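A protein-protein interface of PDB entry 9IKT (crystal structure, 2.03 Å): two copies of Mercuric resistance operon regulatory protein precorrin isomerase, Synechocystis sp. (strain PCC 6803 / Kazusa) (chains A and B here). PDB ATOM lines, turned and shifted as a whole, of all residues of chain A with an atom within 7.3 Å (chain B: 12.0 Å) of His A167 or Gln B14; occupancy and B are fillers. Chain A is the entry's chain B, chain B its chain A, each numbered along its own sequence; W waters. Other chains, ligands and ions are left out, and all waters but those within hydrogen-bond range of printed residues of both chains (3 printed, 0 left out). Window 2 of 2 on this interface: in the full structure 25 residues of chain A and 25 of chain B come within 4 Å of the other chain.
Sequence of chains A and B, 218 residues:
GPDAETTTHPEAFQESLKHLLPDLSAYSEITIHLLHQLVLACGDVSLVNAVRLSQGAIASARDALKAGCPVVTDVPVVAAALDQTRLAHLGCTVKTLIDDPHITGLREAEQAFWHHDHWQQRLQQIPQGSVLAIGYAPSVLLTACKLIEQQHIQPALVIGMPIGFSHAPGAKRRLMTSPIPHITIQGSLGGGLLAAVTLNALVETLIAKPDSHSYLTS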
ATOM      1  N   TYR A 136      -3.851   8.271 -29.102  1.00  0.00           N
ATOM      2  CA  TYR A 136      -4.873   7.915 -28.123  1.00  0.00           C
ATOM      3  C   TYR A 136      -4.866   8.798 -26.874  1.00  0.00           C
ATOM      4  O   TYR A 136      -5.876   9.433 -26.578  1.00  0.00           O
ATOM      5  CB  TYR A 136      -4.723   6.444 -27.710  1.00  0.00           C
ATOM      6  CG  TYR A 136      -5.844   5.944 -26.819  1.00  0.00           C
ATOM      7  CD1 TYR A 136      -7.099   5.665 -27.340  1.00  0.00           C
ATOM      8  CD2 TYR A 136      -5.653   5.784 -25.449  1.00  0.00           C
ATOM      9  CE1 TYR A 136      -8.124   5.209 -26.536  1.00  0.00           C
ATOM     10  CE2 TYR A 136      -6.670   5.328 -24.639  1.00  0.00           C
ATOM     11  CZ  TYR A 136      -7.904   5.040 -25.190  1.00  0.00           C
ATOM     12  OH  TYR A 136      -8.927   4.592 -24.390  1.00  0.00           O
ATOM     13  N   PRO A 138      -4.186  11.722 -24.235  1.00  0.00           N
ATOM     14  CA  PRO A 138      -3.698  13.084 -23.953  1.00  0.00           C
ATOM     15  C   PRO A 138      -2.619  13.139 -22.874  1.00  0.00           C
ATOM     16  O   PRO A 138      -1.718  13.981 -22.960  1.00  0.00           O
ATOM     17  CB  PRO A 138      -4.971  13.824 -23.512  1.00  0.00           C
ATOM     18  CG  PRO A 138      -6.088  13.082 -24.217  1.00  0.00           C
ATOM     19  CD  PRO A 138      -5.658  11.636 -24.219  1.00  0.00           C
ATOM     20  N   SER A 139      -2.670  12.252 -21.876  1.00  0.00           N
ATOM     21  CA  SER A 139      -1.700  12.302 -20.788  1.00  0.00           C
ATOM     22  C   SER A 139      -0.287  12.037 -21.289  1.00  0.00           C
ATOM     23  O   SER A 139       0.675  12.630 -20.787  1.00  0.00           O
ATOM     24  CB  SER A 139      -2.086  11.294 -19.702  1.00  0.00           C
ATOM     25  OG  SER A 139      -2.252  10.000 -20.261  1.00  0.00           O
ATOM     26  N   LEU A 141       0.780  12.805 -24.280  1.00  0.00           N
ATOM     27  CA  LEU A 141       1.168  14.026 -24.974  1.00  0.00           C
ATOM     28  C   LEU A 141       1.584  15.111 -23.984  1.00  0.00           C
ATOM     29  O   LEU A 141       2.596  15.801 -24.189  1.00  0.00           O
ATOM     30  CB  LEU A 141       0.014  14.495 -25.870  1.00  0.00           C
ATOM     31  CG  LEU A 141       0.252  15.775 -26.670  1.00  0.00           C
ATOM     32  CD1 LEU A 141       1.572  15.682 -27.447  1.00  0.00           C
ATOM     33  CD2 LEU A 141      -0.935  16.117 -27.612  1.00  0.00           C
ATOM     34  N   LEU A 142       0.826  15.265 -22.897  1.00  0.00           N
ATOM     35  CA  LEU A 142       1.170  16.262 -21.886  1.00  0.00           C
ATOM     36  C   LEU A 142       2.549  15.996 -21.295  1.00  0.00           C
ATOM     37  O   LEU A 142       3.379  16.906 -21.199  1.00  0.00           O
ATOM     38  CB  LEU A 142       0.112  16.276 -20.782  1.00  0.00           C
ATOM     39  CG  LEU A 142      -1.147  17.080 -21.089  1.00  0.00           C
ATOM     40  CD1 LEU A 142      -2.271  16.650 -20.152  1.00  0.00           C
ATOM     41  CD2 LEU A 142      -0.873  18.578 -20.976  1.00  0.00           C
ATOM     42  N   PRO A 162      -4.301  12.800 -30.109  1.00  0.00           N
ATOM     43  CA  PRO A 162      -5.019  11.920 -29.185  1.00  0.00           C
ATOM     44  C   PRO A 162      -6.525  11.982 -29.412  1.00  0.00           C
ATOM     45  O   PRO A 162      -7.056  12.922 -30.007  1.00  0.00           O
ATOM     46  CB  PRO A 162      -4.651  12.473 -27.804  1.00  0.00           C
ATOM     47  CG  PRO A 162      -4.440  13.980 -28.081  1.00  0.00           C
ATOM     48  CD  PRO A 162      -3.773  14.016 -29.428  1.00  0.00           C
ATOM     49  N   ILE A 163      -7.207  10.939 -28.926  1.00  0.00           N
ATOM     50  CA  ILE A 163      -8.667  10.913 -28.895  1.00  0.00           C
ATOM     51  C   ILE A 163      -9.181  12.000 -27.942  1.00  0.00           C
ATOM     52  O   ILE A 163      -8.524  12.351 -26.958  1.00  0.00           O
ATOM     53  CB  ILE A 163      -9.132   9.510 -28.461  1.00  0.00           C
ATOM     54  CG1 ILE A 163      -8.825   8.474 -29.558  1.00  0.00           C
ATOM     55  CG2 ILE A 163     -10.602   9.490 -28.073  1.00  0.00           C
ATOM     56  CD1 ILE A 163      -9.491   8.772 -30.875  1.00  0.00           C
ATOM     57  N   GLY A 164     -10.379  12.524 -28.233  1.00  0.00           N
ATOM     58  CA  GLY A 164     -10.962  13.655 -27.532  1.00  0.00           C
ATOM     59  C   GLY A 164     -11.399  13.446 -26.091  1.00  0.00           C
ATOM     60  O   GLY A 164     -12.513  13.826 -25.716  1.00  0.00           O
ATOM     61  N   PHE A 165     -10.532  12.864 -25.270  1.00  0.00           N
ATOM     62  CA  PHE A 165     -10.810  12.794 -23.847  1.00  0.00           C
ATOM     63  C   PHE A 165     -10.702  14.189 -23.228  1.00  0.00           C
ATOM     64  O   PHE A 165     -10.253  15.148 -23.862  1.00  0.00           O
ATOM     65  CB  PHE A 165      -9.846  11.828 -23.163  1.00  0.00           C
ATOM     66  CG  PHE A 165      -9.996  10.401 -23.614  1.00  0.00           C
ATOM     67  CD1 PHE A 165     -11.055   9.629 -23.172  1.00  0.00           C
ATOM     68  CD2 PHE A 165      -9.068   9.835 -24.470  1.00  0.00           C
ATOM     69  CE1 PHE A 165     -11.183   8.311 -23.577  1.00  0.00           C
ATOM     70  CE2 PHE A 165      -9.184   8.529 -24.872  1.00  0.00           C
ATOM     71  CZ  PHE A 165     -10.243   7.763 -24.438  1.00  0.00           C
ATOM     72  N   SER A 166     -11.110  14.282 -21.957  1.00  0.00           N
ATOM     73  CA  SER A 166     -11.304  15.577 -21.309  1.00  0.00           C
ATOM     74  C   SER A 166     -10.060  16.458 -21.355  1.00  0.00           C
ATOM     75  O   SER A 166     -10.179  17.687 -21.423  1.00  0.00           O
ATOM     76  CB  SER A 166     -11.736  15.367 -19.859  1.00  0.00           C
ATOM     77  OG  SER A 166     -10.690  14.752 -19.133  1.00  0.00           O
ATOM     78  N   HIS A 167      -8.870  15.865 -21.305  1.00  0.00           N
ATOM     79  CA  HIS A 167      -7.622  16.620 -21.282  1.00  0.00           C
ATOM     80  C   HIS A 167      -7.017  16.848 -22.663  1.00  0.00           C
ATOM     81  O   HIS A 167      -5.947  17.460 -22.750  1.00  0.00           O
ATOM     82  CB  HIS A 167      -6.585  15.908 -20.411  1.00  0.00           C
ATOM     83  CG  HIS A 167      -6.822  16.056 -18.944  1.00  0.00           C
ATOM     84  ND1 HIS A 167      -8.085  16.067 -18.390  1.00  0.00           N
ATOM     85  CD2 HIS A 167      -5.959  16.235 -17.916  1.00  0.00           C
ATOM     86  CE1 HIS A 167      -7.989  16.231 -17.081  1.00  0.00           C
ATOM     87  NE2 HIS A 167      -6.708  16.332 -16.769  1.00  0.00           N
ATOM     88  N   ALA A 168      -7.650  16.363 -23.732  1.00  0.00           N
ATOM     89  CA  ALA A 168      -7.036  16.487 -25.054  1.00  0.00           C
ATOM     90  C   ALA A 168      -6.884  17.924 -25.543  1.00  0.00           C
ATOM     91  O   ALA A 168      -5.832  18.232 -26.133  1.00  0.00           O
ATOM     92  CB  ALA A 168      -7.821  15.660 -26.086  1.00  0.00           C
ATOM     93  N   PRO A 169      -7.860  18.825 -25.395  1.00  0.00           N
ATOM     94  CA  PRO A 169      -7.631  20.187 -25.895  1.00  0.00           C
ATOM     95  C   PRO A 169      -6.442  20.852 -25.228  1.00  0.00           C
ATOM     96  O   PRO A 169      -5.636  21.497 -25.914  1.00  0.00           O
ATOM     97  CB  PRO A 169      -8.953  20.901 -25.587  1.00  0.00           C
ATOM     98  CG  PRO A 169      -9.967  19.776 -25.549  1.00  0.00           C
ATOM     99  CD  PRO A 169      -9.235  18.662 -24.889  1.00  0.00           C
ATOM    100  N   GLY A 170      -6.294  20.677 -23.913  1.00  0.00           N
ATOM    101  CA  GLY A 170      -5.133  21.222 -23.227  1.00  0.00           C
ATOM    102  C   GLY A 170      -3.821  20.624 -23.702  1.00  0.00           C
ATOM    103  O   GLY A 170      -2.836  21.342 -23.892  1.00  0.00           O
ATOM    104  N   ALA A 171      -3.787  19.299 -23.911  1.00  0.00           N
ATOM    105  CA  ALA A 171      -2.551  18.654 -24.345  1.00  0.00           C
ATOM    106  C   ALA A 171      -2.123  19.164 -25.710  1.00  0.00           C
ATOM    107  O   ALA A 171      -0.935  19.418 -25.949  1.00  0.00           O
ATOM    108  CB  ALA A 171      -2.727  17.128 -24.388  1.00  0.00           C
ATOM    109  N   LYS A 172      -3.077  19.323 -26.625  1.00  0.00           N
ATOM    110  CA  LYS A 172      -2.710  19.755 -27.965  1.00  0.00           C
ATOM    111  C   LYS A 172      -2.345  21.230 -28.001  1.00  0.00           C
ATOM    112  O   LYS A 172      -1.528  21.637 -28.831  1.00  0.00           O
ATOM    113  CB  LYS A 172      -3.844  19.431 -28.944  1.00  0.00           C
ATOM    114  CG  LYS A 172      -4.036  17.911 -29.102  1.00  0.00           C
ATOM    115  CD  LYS A 172      -4.879  17.556 -30.321  1.00  0.00           C
ATOM    116  CE  LYS A 172      -6.320  17.973 -30.138  1.00  0.00           C
ATOM    117  NZ  LYS A 172      -7.169  17.619 -31.314  1.00  0.00           N
ATOM    118  N   ARG A 173      -2.902  22.038 -27.092  1.00  0.00           N
ATOM    119  CA  ARG A 173      -2.461  23.428 -26.977  1.00  0.00           C
ATOM    120  C   ARG A 173      -1.007  23.512 -26.517  1.00  0.00           C
ATOM    121  O   ARG A 173      -0.241  24.351 -27.012  1.00  0.00           O
ATOM    122  CB  ARG A 173      -3.373  24.205 -26.016  1.00  0.00           C
ATOM    123  CG  ARG A 173      -4.744  24.587 -26.585  1.00  0.00           C
ATOM    124  CD  ARG A 173      -5.442  25.628 -25.712  1.00  0.00           C
ATOM    125  NE  ARG A 173      -5.967  25.055 -24.478  1.00  0.00           N
ATOM    126  CZ  ARG A 173      -7.167  24.497 -24.363  1.00  0.00           C
ATOM    127  NH1 ARG A 173      -8.007  24.436 -25.386  1.00  0.00           N
ATOM    128  NH2 ARG A 173      -7.538  23.998 -23.189  1.00  0.00           N
ATOM    129  N   GLN B  14     -10.551   8.366 -16.830  1.00  0.00           N
ATOM    130  CA  GLN B  14     -10.057   9.550 -17.529  1.00  0.00           C
ATOM    131  C   GLN B  14      -9.860   9.272 -19.015  1.00  0.00           C
ATOM    132  O   GLN B  14     -10.354  10.013 -19.867  1.00  0.00           O
ATOM    133  CB  GLN B  14      -8.750  10.035 -16.910  1.00  0.00           C
ATOM    134  CG  GLN B  14      -8.249  11.326 -17.526  1.00  0.00           C
ATOM    135  CD  GLN B  14      -6.913  11.782 -16.963  1.00  0.00           C
ATOM    136  OE1 GLN B  14      -5.840  11.328 -17.380  1.00  0.00           O
ATOM    137  NE2 GLN B  14      -6.978  12.673 -15.986  1.00  0.00           N
ATOM    138  N   GLU B  15      -9.142   8.197 -19.325  1.00  0.00           N
ATOM    139  CA  GLU B  15      -8.892   7.861 -20.716  1.00  0.00           C
ATOM    140  C   GLU B  15      -9.469   6.489 -21.049  1.00  0.00           C
ATOM    141  O   GLU B  15      -8.792   5.622 -21.613  1.00  0.00           O
ATOM    142  CB  GLU B  15      -7.399   7.971 -21.004  1.00  0.00           C
ATOM    143  CG  GLU B  15      -6.997   9.441 -21.104  1.00  0.00           C
ATOM    144  CD  GLU B  15      -5.515   9.674 -21.016  1.00  0.00           C
ATOM    145  OE1 GLU B  15      -4.760   8.697 -20.890  1.00  0.00           O
ATOM    146  OE2 GLU B  15      -5.093  10.846 -21.090  1.00  0.00           O
ATOM    147  N   SER B  16     -10.746   6.316 -20.725  1.00  0.00           N
ATOM    148  CA  SER B  16     -11.504   5.107 -21.018  1.00  0.00           C
ATOM    149  C   SER B  16     -12.504   5.409 -22.125  1.00  0.00           C
ATOM    150  O   SER B  16     -13.325   6.323 -21.989  1.00  0.00           O
ATOM    151  CB  SER B  16     -12.232   4.611 -19.771  1.00  0.00           C
ATOM    152  OG  SER B  16     -13.382   3.862 -20.145  1.00  0.00           O
ATOM    153  N   LEU B  17     -12.447   4.630 -23.204  1.00  0.00           N
ATOM    154  CA  LEU B  17     -13.302   4.905 -24.355  1.00  0.00           C
ATOM    155  C   LEU B  17     -14.769   4.636 -24.042  1.00  0.00           C
ATOM    156  O   LEU B  17     -15.645   5.385 -24.490  1.00  0.00           O
ATOM    157  CB  LEU B  17     -12.850   4.076 -25.557  1.00  0.00           C
ATOM    158  CG  LEU B  17     -13.451   4.461 -26.908  1.00  0.00           C
ATOM    159  CD1 LEU B  17     -13.216   5.924 -27.257  1.00  0.00           C
ATOM    160  CD2 LEU B  17     -12.917   3.547 -28.005  1.00  0.00           C
ATOM    161  N   LYS B  18     -15.061   3.572 -23.283  1.00  0.00           N
ATOM    162  CA  LYS B  18     -16.454   3.285 -22.944  1.00  0.00           C
ATOM    163  C   LYS B  18     -17.058   4.411 -22.108  1.00  0.00           C
ATOM    164  O   LYS B  18     -18.257   4.699 -22.211  1.00  0.00           O
ATOM    165  CB  LYS B  18     -16.567   1.947 -22.203  1.00  0.00           C
ATOM    166  N   HIS B  19     -16.244   5.082 -21.308  1.00  0.00           N
ATOM    167  CA  HIS B  19     -16.747   6.192 -20.510  1.00  0.00           C
ATOM    168  C   HIS B  19     -16.790   7.505 -21.281  1.00  0.00           C
ATOM    169  O   HIS B  19     -17.495   8.427 -20.861  1.00  0.00           O
ATOM    170  CB  HIS B  19     -15.896   6.308 -19.253  1.00  0.00           C
ATOM    171  CG  HIS B  19     -16.005   5.115 -18.355  1.00  0.00           C
ATOM    172  ND1 HIS B  19     -15.098   4.077 -18.383  1.00  0.00           N
ATOM    173  CD2 HIS B  19     -16.890   4.814 -17.374  1.00  0.00           C
ATOM    174  CE1 HIS B  19     -15.436   3.174 -17.476  1.00  0.00           C
ATOM    175  NE2 HIS B  19     -16.518   3.600 -16.847  1.00  0.00           N
ATOM    176  N   LEU B  20     -16.062   7.610 -22.397  1.00  0.00           N
ATOM    177  CA  LEU B  20     -16.187   8.769 -23.280  1.00  0.00           C
ATOM    178  C   LEU B  20     -17.415   8.672 -24.184  1.00  0.00           C
ATOM    179  O   LEU B  20     -18.067   9.685 -24.465  1.00  0.00           O
ATOM    180  CB  LEU B  20     -14.938   8.902 -24.142  1.00  0.00           C
ATOM    181  CG  LEU B  20     -15.009   9.917 -25.273  1.00  0.00           C
ATOM    182  CD1 LEU B  20     -15.107  11.312 -24.704  1.00  0.00           C
ATOM    183  CD2 LEU B  20     -13.801   9.772 -26.186  1.00  0.00           C
ATOM    184  N   LEU B  21     -17.727   7.479 -24.671  1.00  0.00           N
ATOM    185  CA  LEU B  21     -18.872   7.301 -25.547  1.00  0.00           C
ATOM    186  C   LEU B  21     -20.166   7.220 -24.746  1.00  0.00           C
ATOM    187  O   LEU B  21     -20.161   6.841 -23.573  1.00  0.00           O
ATOM    188  CB  LEU B  21     -18.703   6.033 -26.377  1.00  0.00           C
ATOM    189  CG  LEU B  21     -17.489   6.093 -27.301  1.00  0.00           C
ATOM    190  CD1 LEU B  21     -17.354   4.828 -28.127  1.00  0.00           C
ATOM    191  CD2 LEU B  21     -17.591   7.311 -28.175  1.00  0.00           C
ATOM    192  N   LEU B  40     -12.023   5.020 -32.615  1.00  0.00           N
ATOM    193  CA  LEU B  40     -10.569   4.952 -32.542  1.00  0.00           C
ATOM    194  C   LEU B  40      -9.921   5.252 -33.889  1.00  0.00           C
ATOM    195  O   LEU B  40      -8.807   5.776 -33.927  1.00  0.00           O
ATOM    196  CB  LEU B  40     -10.128   3.575 -32.052  1.00  0.00           C
ATOM    197  CG  LEU B  40     -10.376   3.192 -30.590  1.00  0.00           C
ATOM    198  CD1 LEU B  40      -9.978   1.733 -30.373  1.00  0.00           C
ATOM    199  CD2 LEU B  40      -9.614   4.072 -29.625  1.00  0.00           C
ATOM    200  N   VAL B  45     -16.458  10.984 -32.215  1.00  0.00           N
ATOM    201  CA  VAL B  45     -17.371  10.313 -31.297  1.00  0.00           C
ATOM    202  C   VAL B  45     -18.783  10.251 -31.864  1.00  0.00           C
ATOM    203  O   VAL B  45     -19.565   9.359 -31.517  1.00  0.00           O
ATOM    204  CB  VAL B  45     -17.331  11.030 -29.934  1.00  0.00           C
ATOM    205  CG1 VAL B  45     -18.413  10.504 -29.022  1.00  0.00           C
ATOM    206  CG2 VAL B  45     -15.966  10.853 -29.290  1.00  0.00           C
HETATM  207  O   HOH W   1     -12.337  11.907 -20.661  1.00  0.00           O
HETATM  208  O   HOH W   2     -10.573   2.433 -23.574  1.00  0.00           O
HETATM  209  O   HOH W   3      -7.400  12.889 -20.636  1.00  0.00           O
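Water W2 bridges the side-chain hydroxyl of Tyr A136 (2.8 Å) and the backbone NH of Leu B17 (2.9 Å). Water W1 bridges O of Gln B14 and N of Ser A166. Water W3 lies within hydrogen-bond range of OE2 of Glu B15 (3.1 Å) and N of His A167 (3.4 Å).
Among the printed residues, merely in contact across the chains: Phe A165 with Ser B16 (3.3 Å), Phe A165 with Gln B14 (3.4 Å), Phe A165 with Glu B15 (3.6 Å), Tyr A136 with Leu B40 (3.6 Å), Tyr A136 with Leu B17 (3.7 Å), Ile A163 with Leu B20 (3.7 Å), Gly A164 with Leu B20 (3.8 Å), His A167 with Gln B14 (3.8 Å), Phe A165 with Leu B20 (3.8 Å) and Phe A165 with Leu B17 (3.9 Å).
Of the printed residues of chain B, His A167 touches Gln B14 (3.8 Å). Printed residues of chain A within 4 Å of Gln B14: Phe A165 and His A167. Pro A138 touches one residue of chain B. Of chain B, only Glu B15 comes within 4 Å of Ser A139. Of chain B, only Leu B20 comes within 4 Å of Gly A164. No residue of chain B comes within 4 Å of Ser A166. No residue of chain B comes within 4 Å of Ala A168. No residue of chain B comes within 4 Å of Pro A169. No residue of chain B comes within 4 Å of Ala A171. Of the printed residues of chain A, Glu B15 touches Tyr A136, Pro A138, Ser A139 and Phe A165. Of the printed residues of chain A, Leu B20 touches Ile A163 (3.7 Å), Gly A164 (3.8 Å) and Phe A165 (3.8 Å). Of the printed residues of chain A, Leu B17 touches Tyr A136 and Phe A165. Of the printed residues of chain A, Leu B40 touches Tyr A136. Lys B18 touches none of the printed residues of chain A. Leu A141 touches none of the printed residues of chain B. The nearest residue of chain B that does not touch His A167 is Glu B15 (5.3 Å). The nearest residue of chain A that does not touch Gln B14 is Ser A139 (4.4 Å).
No position is printed for both chains. Of the 13 pairs that touch across the chains among the printed residues, none has its exchanged pair printed and touching as well.
Hydrophobic or aromatic side chains of chain A that line the printed part of chain B: Tyr A136, Pro A138, Ile A163, Phe A165 and His A167. Hydrophobic or aromatic side chains of chain B that line the printed part of chain A: Leu B20 and Leu B40. Among the printed residues, no Asp or Glu carboxylate lies within 4 Å of a Lys or Arg side-chain nitrogen of the other chain.
N of Ile A163 sits at hydrogen-bond distance from O of Tyr A136, at 3.1 Å. ND1 of His B19 is in hydrogen-bond range of OG of Ser B16, 2.5 Å away. A ring nitrogen (ND1) of His A167 is in hydrogen-bond range of the side-chain hydroxyl (OG) of Ser A166.
OG of Ser A139 lies within hydrogen-bond range of OE1 of Glu B15. The backbone nitrogen (N) of Pro A138 sits close to the side-chain carboxylate (OE2) of Glu B15 (3.4 Å). O of Glu B15 lies within hydrogen-bond range of OH of Tyr A136 (3.0 Å).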
